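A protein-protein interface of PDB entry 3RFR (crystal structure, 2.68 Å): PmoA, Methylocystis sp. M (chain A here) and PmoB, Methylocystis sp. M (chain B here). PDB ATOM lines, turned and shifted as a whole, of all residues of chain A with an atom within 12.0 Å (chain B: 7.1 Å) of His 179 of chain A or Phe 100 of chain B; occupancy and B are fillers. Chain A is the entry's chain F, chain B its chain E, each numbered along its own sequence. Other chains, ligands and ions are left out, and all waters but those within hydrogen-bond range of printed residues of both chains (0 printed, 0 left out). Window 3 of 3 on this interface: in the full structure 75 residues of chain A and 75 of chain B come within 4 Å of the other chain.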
ATOM      1  N   ALA A 175      26.412 -13.728 -35.272  1.00  0.00           N
ATOM      2  CA  ALA A 175      25.649 -14.871 -34.873  1.00  0.00           C
ATOM      3  C   ALA A 175      26.186 -16.173 -35.481  1.00  0.00           C
ATOM      4  O   ALA A 175      26.803 -16.200 -36.572  1.00  0.00           O
ATOM      5  CB  ALA A 175      24.183 -14.663 -35.259  1.00  0.00           C
ATOM      6  N   THR A 176      25.938 -17.253 -34.751  1.00  0.00           N
ATOM      7  CA  THR A 176      26.281 -18.577 -35.210  1.00  0.00           C
ATOM      8  C   THR A 176      25.223 -19.540 -34.686  1.00  0.00           C
ATOM      9  O   THR A 176      24.689 -19.345 -33.597  1.00  0.00           O
ATOM     10  CB  THR A 176      27.725 -19.003 -34.765  1.00  0.00           C
ATOM     11  OG1 THR A 176      28.090 -20.238 -35.409  1.00  0.00           O
ATOM     12  CG2 THR A 176      27.799 -19.164 -33.268  1.00  0.00           C
ATOM     13  N   GLU A 177      24.910 -20.556 -35.478  1.00  0.00           N
ATOM     14  CA  GLU A 177      23.985 -21.568 -35.044  1.00  0.00           C
ATOM     15  C   GLU A 177      24.750 -22.785 -34.646  1.00  0.00           C
ATOM     16  O   GLU A 177      25.403 -23.403 -35.465  1.00  0.00           O
ATOM     17  CB  GLU A 177      23.026 -21.956 -36.148  1.00  0.00           C
ATOM     18  CG  GLU A 177      21.983 -22.887 -35.664  1.00  0.00           C
ATOM     19  CD  GLU A 177      21.732 -24.008 -36.623  1.00  0.00           C
ATOM     20  OE1 GLU A 177      21.196 -23.725 -37.716  1.00  0.00           O
ATOM     21  OE2 GLU A 177      22.068 -25.166 -36.283  1.00  0.00           O
ATOM     22  N   GLN A 178      24.651 -23.141 -33.383  1.00  0.00           N
ATOM     23  CA  GLN A 178      25.306 -24.321 -32.900  1.00  0.00           C
ATOM     24  C   GLN A 178      24.232 -25.262 -32.426  1.00  0.00           C
ATOM     25  O   GLN A 178      23.450 -24.899 -31.545  1.00  0.00           O
ATOM     26  CB  GLN A 178      26.250 -23.972 -31.768  1.00  0.00           C
ATOM     27  CG  GLN A 178      27.400 -23.083 -32.200  1.00  0.00           C
ATOM     28  CD  GLN A 178      28.393 -23.800 -33.084  1.00  0.00           C
ATOM     29  OE1 GLN A 178      28.680 -23.340 -34.172  1.00  0.00           O
ATOM     30  NE2 GLN A 178      28.926 -24.932 -32.617  1.00  0.00           N
ATOM     31  N   HIS A 179      24.180 -26.446 -33.052  1.00  0.00           N
ATOM     32  CA  HIS A 179      23.314 -27.534 -32.654  1.00  0.00           C
ATOM     33  C   HIS A 179      21.897 -27.110 -32.383  1.00  0.00           C
ATOM     34  O   HIS A 179      21.303 -27.535 -31.389  1.00  0.00           O
ATOM     35  CB  HIS A 179      23.890 -28.261 -31.453  1.00  0.00           C
ATOM     36  CG  HIS A 179      25.101 -29.066 -31.784  1.00  0.00           C
ATOM     37  ND1 HIS A 179      26.384 -28.600 -31.585  1.00  0.00           N
ATOM     38  CD2 HIS A 179      25.230 -30.309 -32.307  1.00  0.00           C
ATOM     39  CE1 HIS A 179      27.254 -29.513 -31.981  1.00  0.00           C
ATOM     40  NE2 HIS A 179      26.578 -30.565 -32.410  1.00  0.00           N
ATOM     41  N   GLY A 180      21.369 -26.275 -33.275  1.00  0.00           N
ATOM     42  CA  GLY A 180      19.965 -25.879 -33.248  1.00  0.00           C
ATOM     43  C   GLY A 180      19.678 -24.638 -32.426  1.00  0.00           C
ATOM     44  O   GLY A 180      18.518 -24.299 -32.202  1.00  0.00           O
ATOM     45  N   GLN A 181      20.722 -23.945 -31.997  1.00  0.00           N
ATOM     46  CA  GLN A 181      20.591 -22.943 -30.964  1.00  0.00           C
ATOM     47  C   GLN A 181      21.447 -21.747 -31.318  1.00  0.00           C
ATOM     48  O   GLN A 181      22.565 -21.889 -31.839  1.00  0.00           O
ATOM     49  CB  GLN A 181      21.055 -23.579 -29.674  1.00  0.00           C
ATOM     50  CG  GLN A 181      21.373 -22.689 -28.552  1.00  0.00           C
ATOM     51  CD  GLN A 181      21.225 -23.411 -27.238  1.00  0.00           C
ATOM     52  OE1 GLN A 181      20.456 -24.363 -27.133  1.00  0.00           O
ATOM     53  NE2 GLN A 181      21.948 -22.957 -26.220  1.00  0.00           N
ATOM     54  N   LEU A 182      20.922 -20.559 -31.056  1.00  0.00           N
ATOM     55  CA  LEU A 182      21.656 -19.333 -31.381  1.00  0.00           C
ATOM     56  C   LEU A 182      22.671 -18.977 -30.302  1.00  0.00           C
ATOM     57  O   LEU A 182      22.371 -19.039 -29.113  1.00  0.00           O
ATOM     58  CB  LEU A 182      20.689 -18.164 -31.623  1.00  0.00           C
ATOM     59  CG  LEU A 182      21.263 -16.873 -32.228  1.00  0.00           C
ATOM     60  CD1 LEU A 182      21.677 -17.044 -33.691  1.00  0.00           C
ATOM     61  CD2 LEU A 182      20.214 -15.787 -32.057  1.00  0.00           C
ATOM     62  N   MET A 183      23.862 -18.604 -30.750  1.00  0.00           N
ATOM     63  CA  MET A 183      24.934 -18.151 -29.880  1.00  0.00           C
ATOM     64  C   MET A 183      25.664 -16.970 -30.548  1.00  0.00           C
ATOM     65  O   MET A 183      25.733 -16.890 -31.796  1.00  0.00           O
ATOM     66  CB  MET A 183      25.929 -19.296 -29.650  1.00  0.00           C
ATOM     67  CG  MET A 183      25.376 -20.428 -28.836  1.00  0.00           C
ATOM     68  SD  MET A 183      26.577 -21.718 -28.429  1.00  0.00           S
ATOM     69  CE  MET A 183      27.533 -20.981 -27.107  1.00  0.00           C
ATOM     70  N   THR A 184      26.200 -16.063 -29.747  1.00  0.00           N
ATOM     71  CA  THR A 184      27.157 -15.120 -30.290  1.00  0.00           C
ATOM     72  C   THR A 184      28.536 -15.777 -30.433  1.00  0.00           C
ATOM     73  O   THR A 184      28.808 -16.777 -29.767  1.00  0.00           O
ATOM     74  CB  THR A 184      27.333 -13.917 -29.372  1.00  0.00           C
ATOM     75  OG1 THR A 184      27.585 -14.379 -28.041  1.00  0.00           O
ATOM     76  CG2 THR A 184      26.095 -13.085 -29.369  1.00  0.00           C
ATOM     77  N   ASP A 187      29.845 -15.984 -26.899  1.00  0.00           N
ATOM     78  CA  ASP A 187      29.400 -17.139 -26.176  1.00  0.00           C
ATOM     79  C   ASP A 187      30.274 -18.329 -26.556  1.00  0.00           C
ATOM     80  O   ASP A 187      30.711 -19.111 -25.689  1.00  0.00           O
ATOM     81  CB  ASP A 187      27.916 -17.419 -26.476  1.00  0.00           C
ATOM     82  CG  ASP A 187      26.983 -16.338 -25.918  1.00  0.00           C
ATOM     83  OD1 ASP A 187      27.094 -16.010 -24.734  1.00  0.00           O
ATOM     84  OD2 ASP A 187      26.115 -15.808 -26.643  1.00  0.00           O
ATOM     85  N   LEU A 188      30.549 -18.448 -27.845  1.00  0.00           N
ATOM     86  CA  LEU A 188      31.268 -19.600 -28.384  1.00  0.00           C
ATOM     87  C   LEU A 188      32.718 -19.615 -27.951  1.00  0.00           C
ATOM     88  O   LEU A 188      33.293 -20.677 -27.708  1.00  0.00           O
ATOM     89  CB  LEU A 188      31.183 -19.643 -29.924  1.00  0.00           C
ATOM     90  CG  LEU A 188      31.209 -21.050 -30.541  1.00  0.00           C
ATOM     91  CD1 LEU A 188      30.240 -22.030 -29.843  1.00  0.00           C
ATOM     92  CD2 LEU A 188      30.862 -20.921 -31.990  1.00  0.00           C
ATOM     93  N   LEU A 191      32.451 -20.903 -24.463  1.00  0.00           N
ATOM     94  CA  LEU A 191      32.256 -22.376 -24.438  1.00  0.00           C
ATOM     95  C   LEU A 191      33.519 -23.142 -24.851  1.00  0.00           C
ATOM     96  O   LEU A 191      33.857 -24.120 -24.192  1.00  0.00           O
ATOM     97  CB  LEU A 191      31.012 -22.876 -25.246  1.00  0.00           C
ATOM     98  CG  LEU A 191      30.704 -24.412 -25.183  1.00  0.00           C
ATOM     99  CD1 LEU A 191      29.692 -24.815 -24.081  1.00  0.00           C
ATOM    100  CD2 LEU A 191      30.312 -25.118 -26.492  1.00  0.00           C
ATOM    101  N   HIS A 192      34.196 -22.688 -25.912  1.00  0.00           N
ATOM    102  CA  HIS A 192      35.299 -23.429 -26.555  1.00  0.00           C
ATOM    103  C   HIS A 192      36.555 -23.503 -25.685  1.00  0.00           C
ATOM    104  O   HIS A 192      37.076 -24.560 -25.403  1.00  0.00           O
ATOM    105  CB  HIS A 192      35.713 -22.760 -27.885  1.00  0.00           C
ATOM    106  CG  HIS A 192      35.030 -23.285 -29.123  1.00  0.00           C
ATOM    107  ND1 HIS A 192      33.668 -23.508 -29.206  1.00  0.00           N
ATOM    108  CD2 HIS A 192      35.529 -23.557 -30.358  1.00  0.00           C
ATOM    109  CE1 HIS A 192      33.366 -23.925 -30.427  1.00  0.00           C
ATOM    110  NE2 HIS A 192      34.478 -23.961 -31.146  1.00  0.00           N
ATOM    111  N   VAL A 194      38.034 -23.746 -22.704  1.00  0.00           N
ATOM    112  CA  VAL A 194      37.440 -24.107 -21.408  1.00  0.00           C
ATOM    113  C   VAL A 194      38.164 -23.511 -20.216  1.00  0.00           C
ATOM    114  O   VAL A 194      39.339 -23.792 -20.007  1.00  0.00           O
ATOM    115  CB  VAL A 194      37.392 -25.644 -21.215  1.00  0.00           C
ATOM    116  CG1 VAL A 194      36.542 -25.980 -19.989  1.00  0.00           C
ATOM    117  CG2 VAL A 194      36.845 -26.334 -22.455  1.00  0.00           C
ATOM    118  N   LEU B  63      34.190 -37.336 -24.250  1.00  0.00           N
ATOM    119  CA  LEU B  63      34.176 -37.749 -22.875  1.00  0.00           C
ATOM    120  C   LEU B  63      32.702 -37.842 -22.536  1.00  0.00           C
ATOM    121  O   LEU B  63      31.972 -36.864 -22.659  1.00  0.00           O
ATOM    122  CB  LEU B  63      34.957 -36.759 -21.995  1.00  0.00           C
ATOM    123  CG  LEU B  63      34.784 -36.626 -20.466  1.00  0.00           C
ATOM    124  CD1 LEU B  63      34.597 -37.947 -19.744  1.00  0.00           C
ATOM    125  CD2 LEU B  63      35.966 -35.896 -19.871  1.00  0.00           C
ATOM    126  N   GLY B  65      29.403 -40.004 -20.108  1.00  0.00           N
ATOM    127  CA  GLY B  65      29.131 -40.660 -18.842  1.00  0.00           C
ATOM    128  C   GLY B  65      27.728 -40.414 -18.407  1.00  0.00           C
ATOM    129  O   GLY B  65      26.936 -39.869 -19.156  1.00  0.00           O
ATOM    130  N   LEU B  85      27.562 -28.249 -16.803  1.00  0.00           N
ATOM    131  CA  LEU B  85      28.464 -29.338 -17.179  1.00  0.00           C
ATOM    132  C   LEU B  85      29.799 -28.783 -17.712  1.00  0.00           C
ATOM    133  O   LEU B  85      29.828 -27.736 -18.316  1.00  0.00           O
ATOM    134  CB  LEU B  85      27.787 -30.268 -18.215  1.00  0.00           C
ATOM    135  CG  LEU B  85      28.642 -31.336 -18.928  1.00  0.00           C
ATOM    136  CD1 LEU B  85      28.938 -32.484 -17.995  1.00  0.00           C
ATOM    137  CD2 LEU B  85      27.999 -31.832 -20.192  1.00  0.00           C
ATOM    138  N   THR B  97      33.855 -28.320 -28.116  1.00  0.00           N
ATOM    139  CA  THR B  97      33.259 -28.070 -29.411  1.00  0.00           C
ATOM    140  C   THR B  97      31.753 -28.174 -29.300  1.00  0.00           C
ATOM    141  O   THR B  97      31.022 -27.434 -29.949  1.00  0.00           O
ATOM    142  CB  THR B  97      33.886 -29.041 -30.406  1.00  0.00           C
ATOM    143  OG1 THR B  97      34.820 -28.312 -31.198  1.00  0.00           O
ATOM    144  CG2 THR B  97      32.860 -29.782 -31.261  1.00  0.00           C
ATOM    145  N   ALA B  98      31.311 -29.092 -28.443  1.00  0.00           N
ATOM    146  CA  ALA B  98      29.922 -29.189 -28.016  1.00  0.00           C
ATOM    147  C   ALA B  98      29.930 -29.950 -26.717  1.00  0.00           C
ATOM    148  O   ALA B  98      30.970 -30.485 -26.317  1.00  0.00           O
ATOM    149  CB  ALA B  98      29.089 -29.899 -29.038  1.00  0.00           C
ATOM    150  N   GLN B  99      28.785 -29.949 -26.048  1.00  0.00           N
ATOM    151  CA  GLN B  99      28.530 -30.815 -24.928  1.00  0.00           C
ATOM    152  C   GLN B  99      27.020 -30.921 -24.770  1.00  0.00           C
ATOM    153  O   GLN B  99      26.275 -30.086 -25.285  1.00  0.00           O
ATOM    154  CB  GLN B  99      29.193 -30.309 -23.655  1.00  0.00           C
ATOM    155  CG  GLN B  99      28.411 -29.249 -22.870  1.00  0.00           C
ATOM    156  CD  GLN B  99      29.195 -28.622 -21.722  1.00  0.00           C
ATOM    157  OE1 GLN B  99      28.673 -27.761 -21.019  1.00  0.00           O
ATOM    158  NE2 GLN B  99      30.449 -29.038 -21.534  1.00  0.00           N
ATOM    159  N   PHE B 100      26.598 -31.983 -24.075  1.00  0.00           N
ATOM    160  CA  PHE B 100      25.199 -32.387 -23.922  1.00  0.00           C
ATOM    161  C   PHE B 100      24.986 -32.987 -22.538  1.00  0.00           C
ATOM    162  O   PHE B 100      25.867 -33.634 -21.973  1.00  0.00           O
ATOM    163  CB  PHE B 100      24.828 -33.415 -24.992  1.00  0.00           C
ATOM    164  CG  PHE B 100      25.204 -33.003 -26.371  1.00  0.00           C
ATOM    165  CD1 PHE B 100      24.249 -32.480 -27.236  1.00  0.00           C
ATOM    166  CD2 PHE B 100      26.522 -33.122 -26.816  1.00  0.00           C
ATOM    167  CE1 PHE B 100      24.597 -32.067 -28.531  1.00  0.00           C
ATOM    168  CE2 PHE B 100      26.892 -32.726 -28.086  1.00  0.00           C
ATOM    169  CZ  PHE B 100      25.920 -32.182 -28.960  1.00  0.00           C
ATOM    170  N   ILE B 101      23.803 -32.761 -22.003  1.00  0.00           N
ATOM    171  CA  ILE B 101      23.342 -33.387 -20.769  1.00  0.00           C
ATOM    172  C   ILE B 101      21.829 -33.263 -20.813  1.00  0.00           C
ATOM    173  O   ILE B 101      21.302 -32.353 -21.468  1.00  0.00           O
ATOM    174  CB  ILE B 101      23.953 -32.713 -19.478  1.00  0.00           C
ATOM    175  CG1 ILE B 101      23.704 -33.565 -18.214  1.00  0.00           C
ATOM    176  CG2 ILE B 101      23.487 -31.250 -19.307  1.00  0.00           C
ATOM    177  CD1 ILE B 101      24.435 -33.056 -16.970  1.00  0.00           C
ATOM    178  N   GLY B 102      21.123 -34.176 -20.159  1.00  0.00           N
ATOM    179  CA  GLY B 102      19.671 -34.110 -20.196  1.00  0.00           C
ATOM    180  C   GLY B 102      19.177 -34.778 -21.451  1.00  0.00           C
ATOM    181  O   GLY B 102      18.738 -35.901 -21.405  1.00  0.00           O
ATOM    182  N   GLU B 103      19.212 -34.090 -22.564  1.00  0.00           N
ATOM    183  CA  GLU B 103      19.249 -34.725 -23.891  1.00  0.00           C
ATOM    184  C   GLU B 103      19.334 -33.497 -24.777  1.00  0.00           C
ATOM    185  O   GLU B 103      18.749 -33.427 -25.839  1.00  0.00           O
ATOM    186  CB  GLU B 103      18.037 -35.615 -24.209  1.00  0.00           C
ATOM    187  CG  GLU B 103      18.356 -37.128 -24.094  1.00  0.00           C
ATOM    188  CD  GLU B 103      17.120 -38.054 -23.882  1.00  0.00           C
ATOM    189  OE1 GLU B 103      16.113 -37.967 -24.641  1.00  0.00           O
ATOM    190  OE2 GLU B 103      17.181 -38.910 -22.966  1.00  0.00           O
ATOM    191  N   GLN B 104      20.099 -32.533 -24.255  1.00  0.00           N
ATOM    192  CA  GLN B 104      20.148 -31.170 -24.697  1.00  0.00           C
ATOM    193  C   GLN B 104      21.578 -30.719 -24.941  1.00  0.00           C
ATOM    194  O   GLN B 104      22.495 -31.069 -24.194  1.00  0.00           O
ATOM    195  CB  GLN B 104      19.613 -30.296 -23.600  1.00  0.00           C
ATOM    196  CG  GLN B 104      18.113 -30.135 -23.582  1.00  0.00           C
ATOM    197  CD  GLN B 104      17.705 -29.156 -22.470  1.00  0.00           C
ATOM    198  OE1 GLN B 104      16.928 -29.500 -21.577  1.00  0.00           O
ATOM    199  NE2 GLN B 104      18.261 -27.937 -22.506  1.00  0.00           N
ATOM    200  N   PHE B 105      21.766 -29.943 -25.995  1.00  0.00           N
ATOM    201  CA  PHE B 105      22.955 -29.153 -26.137  1.00  0.00           C
ATOM    202  C   PHE B 105      22.978 -28.189 -24.927  1.00  0.00           C
ATOM    203  O   PHE B 105      21.986 -27.528 -24.610  1.00  0.00           O
ATOM    204  CB  PHE B 105      22.867 -28.418 -27.465  1.00  0.00           C
ATOM    205  CG  PHE B 105      24.033 -27.559 -27.777  1.00  0.00           C
ATOM    206  CD1 PHE B 105      25.336 -28.056 -27.712  1.00  0.00           C
ATOM    207  CD2 PHE B 105      23.829 -26.240 -28.176  1.00  0.00           C
ATOM    208  CE1 PHE B 105      26.430 -27.225 -28.026  1.00  0.00           C
ATOM    209  CE2 PHE B 105      24.902 -25.416 -28.497  1.00  0.00           C
ATOM    210  CZ  PHE B 105      26.214 -25.909 -28.412  1.00  0.00           C
ATOM    211  N   ALA B 106      24.093 -28.128 -24.220  1.00  0.00           N
ATOM    212  CA  ALA B 106      24.102 -27.367 -23.016  1.00  0.00           C
ATOM    213  C   ALA B 106      25.286 -26.431 -22.928  1.00  0.00           C
ATOM    214  O   ALA B 106      26.171 -26.649 -22.081  1.00  0.00           O
ATOM    215  CB  ALA B 106      24.076 -28.302 -21.820  1.00  0.00           C
ATOM    216  N   PRO B 107      25.324 -25.377 -23.776  1.00  0.00           N
ATOM    217  CA  PRO B 107      26.363 -24.365 -23.598  1.00  0.00           C
ATOM    218  C   PRO B 107      26.065 -23.446 -22.392  1.00  0.00           C
ATOM    219  O   PRO B 107      26.935 -22.684 -21.952  1.00  0.00           O
ATOM    220  CB  PRO B 107      26.306 -23.584 -24.918  1.00  0.00           C
ATOM    221  CG  PRO B 107      24.954 -23.707 -25.359  1.00  0.00           C
ATOM    222  CD  PRO B 107      24.474 -25.064 -24.933  1.00  0.00           C
ATOM    223  N   ALA B 119      22.346 -38.503 -18.501  1.00  0.00           N
ATOM    224  CA  ALA B 119      23.447 -38.812 -19.444  1.00  0.00           C
ATOM    225  C   ALA B 119      24.118 -37.531 -19.880  1.00  0.00           C
ATOM    226  O   ALA B 119      23.455 -36.535 -20.100  1.00  0.00           O
ATOM    227  CB  ALA B 119      22.916 -39.541 -20.665  1.00  0.00           C
ATOM    228  N   PHE B 120      25.428 -37.540 -20.003  1.00  0.00           N
ATOM    229  CA  PHE B 120      26.137 -36.387 -20.589  1.00  0.00           C
ATOM    230  C   PHE B 120      27.198 -36.834 -21.570  1.00  0.00           C
ATOM    231  O   PHE B 120      27.620 -37.988 -21.565  1.00  0.00           O
ATOM    232  CB  PHE B 120      26.771 -35.500 -19.498  1.00  0.00           C
ATOM    233  CG  PHE B 120      27.856 -36.192 -18.689  1.00  0.00           C
ATOM    234  CD1 PHE B 120      29.160 -36.208 -19.145  1.00  0.00           C
ATOM    235  CD2 PHE B 120      27.550 -36.819 -17.469  1.00  0.00           C
ATOM    236  CE1 PHE B 120      30.149 -36.824 -18.430  1.00  0.00           C
ATOM    237  CE2 PHE B 120      28.533 -37.456 -16.751  1.00  0.00           C
ATOM    238  CZ  PHE B 120      29.843 -37.446 -17.235  1.00  0.00           C
ATOM    239  N   SER B 121      27.634 -35.908 -22.406  1.00  0.00           N
ATOM    240  CA  SER B 121      28.835 -36.109 -23.230  1.00  0.00           C
ATOM    241  C   SER B 121      29.458 -34.766 -23.639  1.00  0.00           C
ATOM    242  O   SER B 121      28.760 -33.758 -23.728  1.00  0.00           O
ATOM    243  CB  SER B 121      28.526 -36.973 -24.451  1.00  0.00           C
ATOM    244  OG  SER B 121      27.386 -36.484 -25.129  1.00  0.00           O
ATOM    245  N   ILE B 122      30.776 -34.768 -23.816  1.00  0.00           N
ATOM    246  CA  ILE B 122      31.522 -33.585 -24.168  1.00  0.00           C
ATOM    247  C   ILE B 122      32.414 -33.986 -25.316  1.00  0.00           C
ATOM    248  O   ILE B 122      33.064 -35.018 -25.224  1.00  0.00           O
ATOM    249  CB  ILE B 122      32.430 -33.078 -23.024  1.00  0.00           C
ATOM    250  CG1 ILE B 122      31.649 -32.901 -21.748  1.00  0.00           C
ATOM    251  CG2 ILE B 122      33.075 -31.743 -23.361  1.00  0.00           C
ATOM    252  CD1 ILE B 122      32.502 -32.897 -20.538  1.00  0.00           C
ATOM    253  N   ASN B 123      32.410 -33.157 -26.379  1.00  0.00           N
ATOM    254  CA  ASN B 123      33.246 -33.267 -27.565  1.00  0.00           C
ATOM    255  C   ASN B 123      34.464 -32.372 -27.424  1.00  0.00           C
ATOM    256  O   ASN B 123      34.341 -31.156 -27.395  1.00  0.00           O
ATOM    257  CB  ASN B 123      32.467 -32.824 -28.807  1.00  0.00           C
ATOM    258  CG  ASN B 123      31.225 -33.658 -29.060  1.00  0.00           C
ATOM    259  OD1 ASN B 123      31.236 -34.861 -28.928  1.00  0.00           O
ATOM    260  ND2 ASN B 123      30.151 -33.004 -29.466  1.00  0.00           N
ATOM    261  N   LEU B 268      15.675 -30.773 -18.238  1.00  0.00           N
ATOM    262  CA  LEU B 268      16.388 -31.857 -18.879  1.00  0.00           C
ATOM    263  C   LEU B 268      15.566 -33.136 -18.888  1.00  0.00           C
ATOM    264  O   LEU B 268      14.591 -33.265 -18.147  1.00  0.00           O
ATOM    265  CB  LEU B 268      17.711 -32.084 -18.165  1.00  0.00           C
ATOM    266  CG  LEU B 268      18.737 -30.942 -18.170  1.00  0.00           C
ATOM    267  CD1 LEU B 268      19.948 -31.294 -17.344  1.00  0.00           C
ATOM    268  CD2 LEU B 268      19.154 -30.522 -19.574  1.00  0.00           C
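Of the 15 printed residues of chain A, 5 touch a printed residue of chain B.
Hydrophobic or aromatic side chains of chain A within 4 Å of the printed part of chain B: His 179, Met 183 and Leu 191.
Of the 20 printed residues of chain B, 4 touch a printed residue of chain A.
Printed residues of chain B that touch a printed residue of chain A: Ala 98, Phe 100, Phe 105 and Pro 107.
Hydrophobic or aromatic side chains of chain B within 4 Å of the printed part of chain A: Ala 98, Phe 100, Phe 105 and Pro 107.
Among the printed residues, no Asp or Glu carboxylate lies within 4 Å of a Lys or Arg side-chain nitrogen of the other chain.
O of Gln 178 of chain A touches CE2 of Phe 105 of chain B (3.4 Å).
His 179 of chain A touches Ala 98 of chain B.
His 179 of chain A touches Phe 100 of chain B.
Phe 105 of chain B touches His 179 of chain A.
CD of Gln 181 of chain A touches CD2 of Phe 105 of chain B (3.96 Å).
NE2 of Gln 181 of chain A touches CG of Pro 107 of chain B, 3.2 Å away.
Pro 107 of chain B touches Met 183 of chain A.
Leu 191 of chain A touches Pro 107 of chain B.
Printed residues of chain B within 4 Å of Gln 178 of chain A: Phe 105 (3.4 Å).
Of chain B, only Ala 98, Phe 100 and Phe 105 come within 4 Å of His 179 of chain A.
Of the printed residues of chain B, Gln 181 of chain A touches Phe 105 (3.96 Å) and Pro 107 (3.2 Å).
Of the printed residues of chain B, Leu 191 of chain A touches Pro 107 (3.4 Å).
No residue of chain A comes within 4 Å of Leu 85 of chain B.
No residue of chain A comes within 4 Å of Thr 97 of chain B.
Of chain A, only His 179 (3.5 Å) comes within 4 Å of Ala 98 of chain B.
Of the printed residues of chain A, Phe 100 of chain B touches His 179.
No residue of chain A comes within 4 Å of Ile 101 of chain B.
No residue of chain A comes within 4 Å of Ala 119 of chain B.
No residue of chain A comes within 4 Å of Phe 120 of chain B.
No residue of chain A comes within 4 Å of Ile 122 of chain B.
No residue of chain A comes within 4 Å of Asn 123 of chain B.
The nearest residue of chain B that does not touch His 179 of chain A is Thr 97 of chain B (4.8 Å).
The nearest residue of chain A that does not touch Phe 100 of chain B is Leu 191 of chain A (7.8 Å).
The backbone carbonyl oxygen (O) of Ala 98 of chain B is in hydrogen-bond range of the backbone NH (N) of Asn 123 of chain B, 3.0 Å away.
N of Phe 100 of chain B sits at hydrogen-bond distance from O of Ser 121 of chain B (2.8 Å).
The side-chain hydroxyl of Thr 176 of chain A is in hydrogen-bond range of the side-chain amide oxygen of Gln 178 of chain A (3.4 Å).
O of Met 183 of chain A lies within hydrogen-bond range of N of Thr 176 of chain A (3.0 Å).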
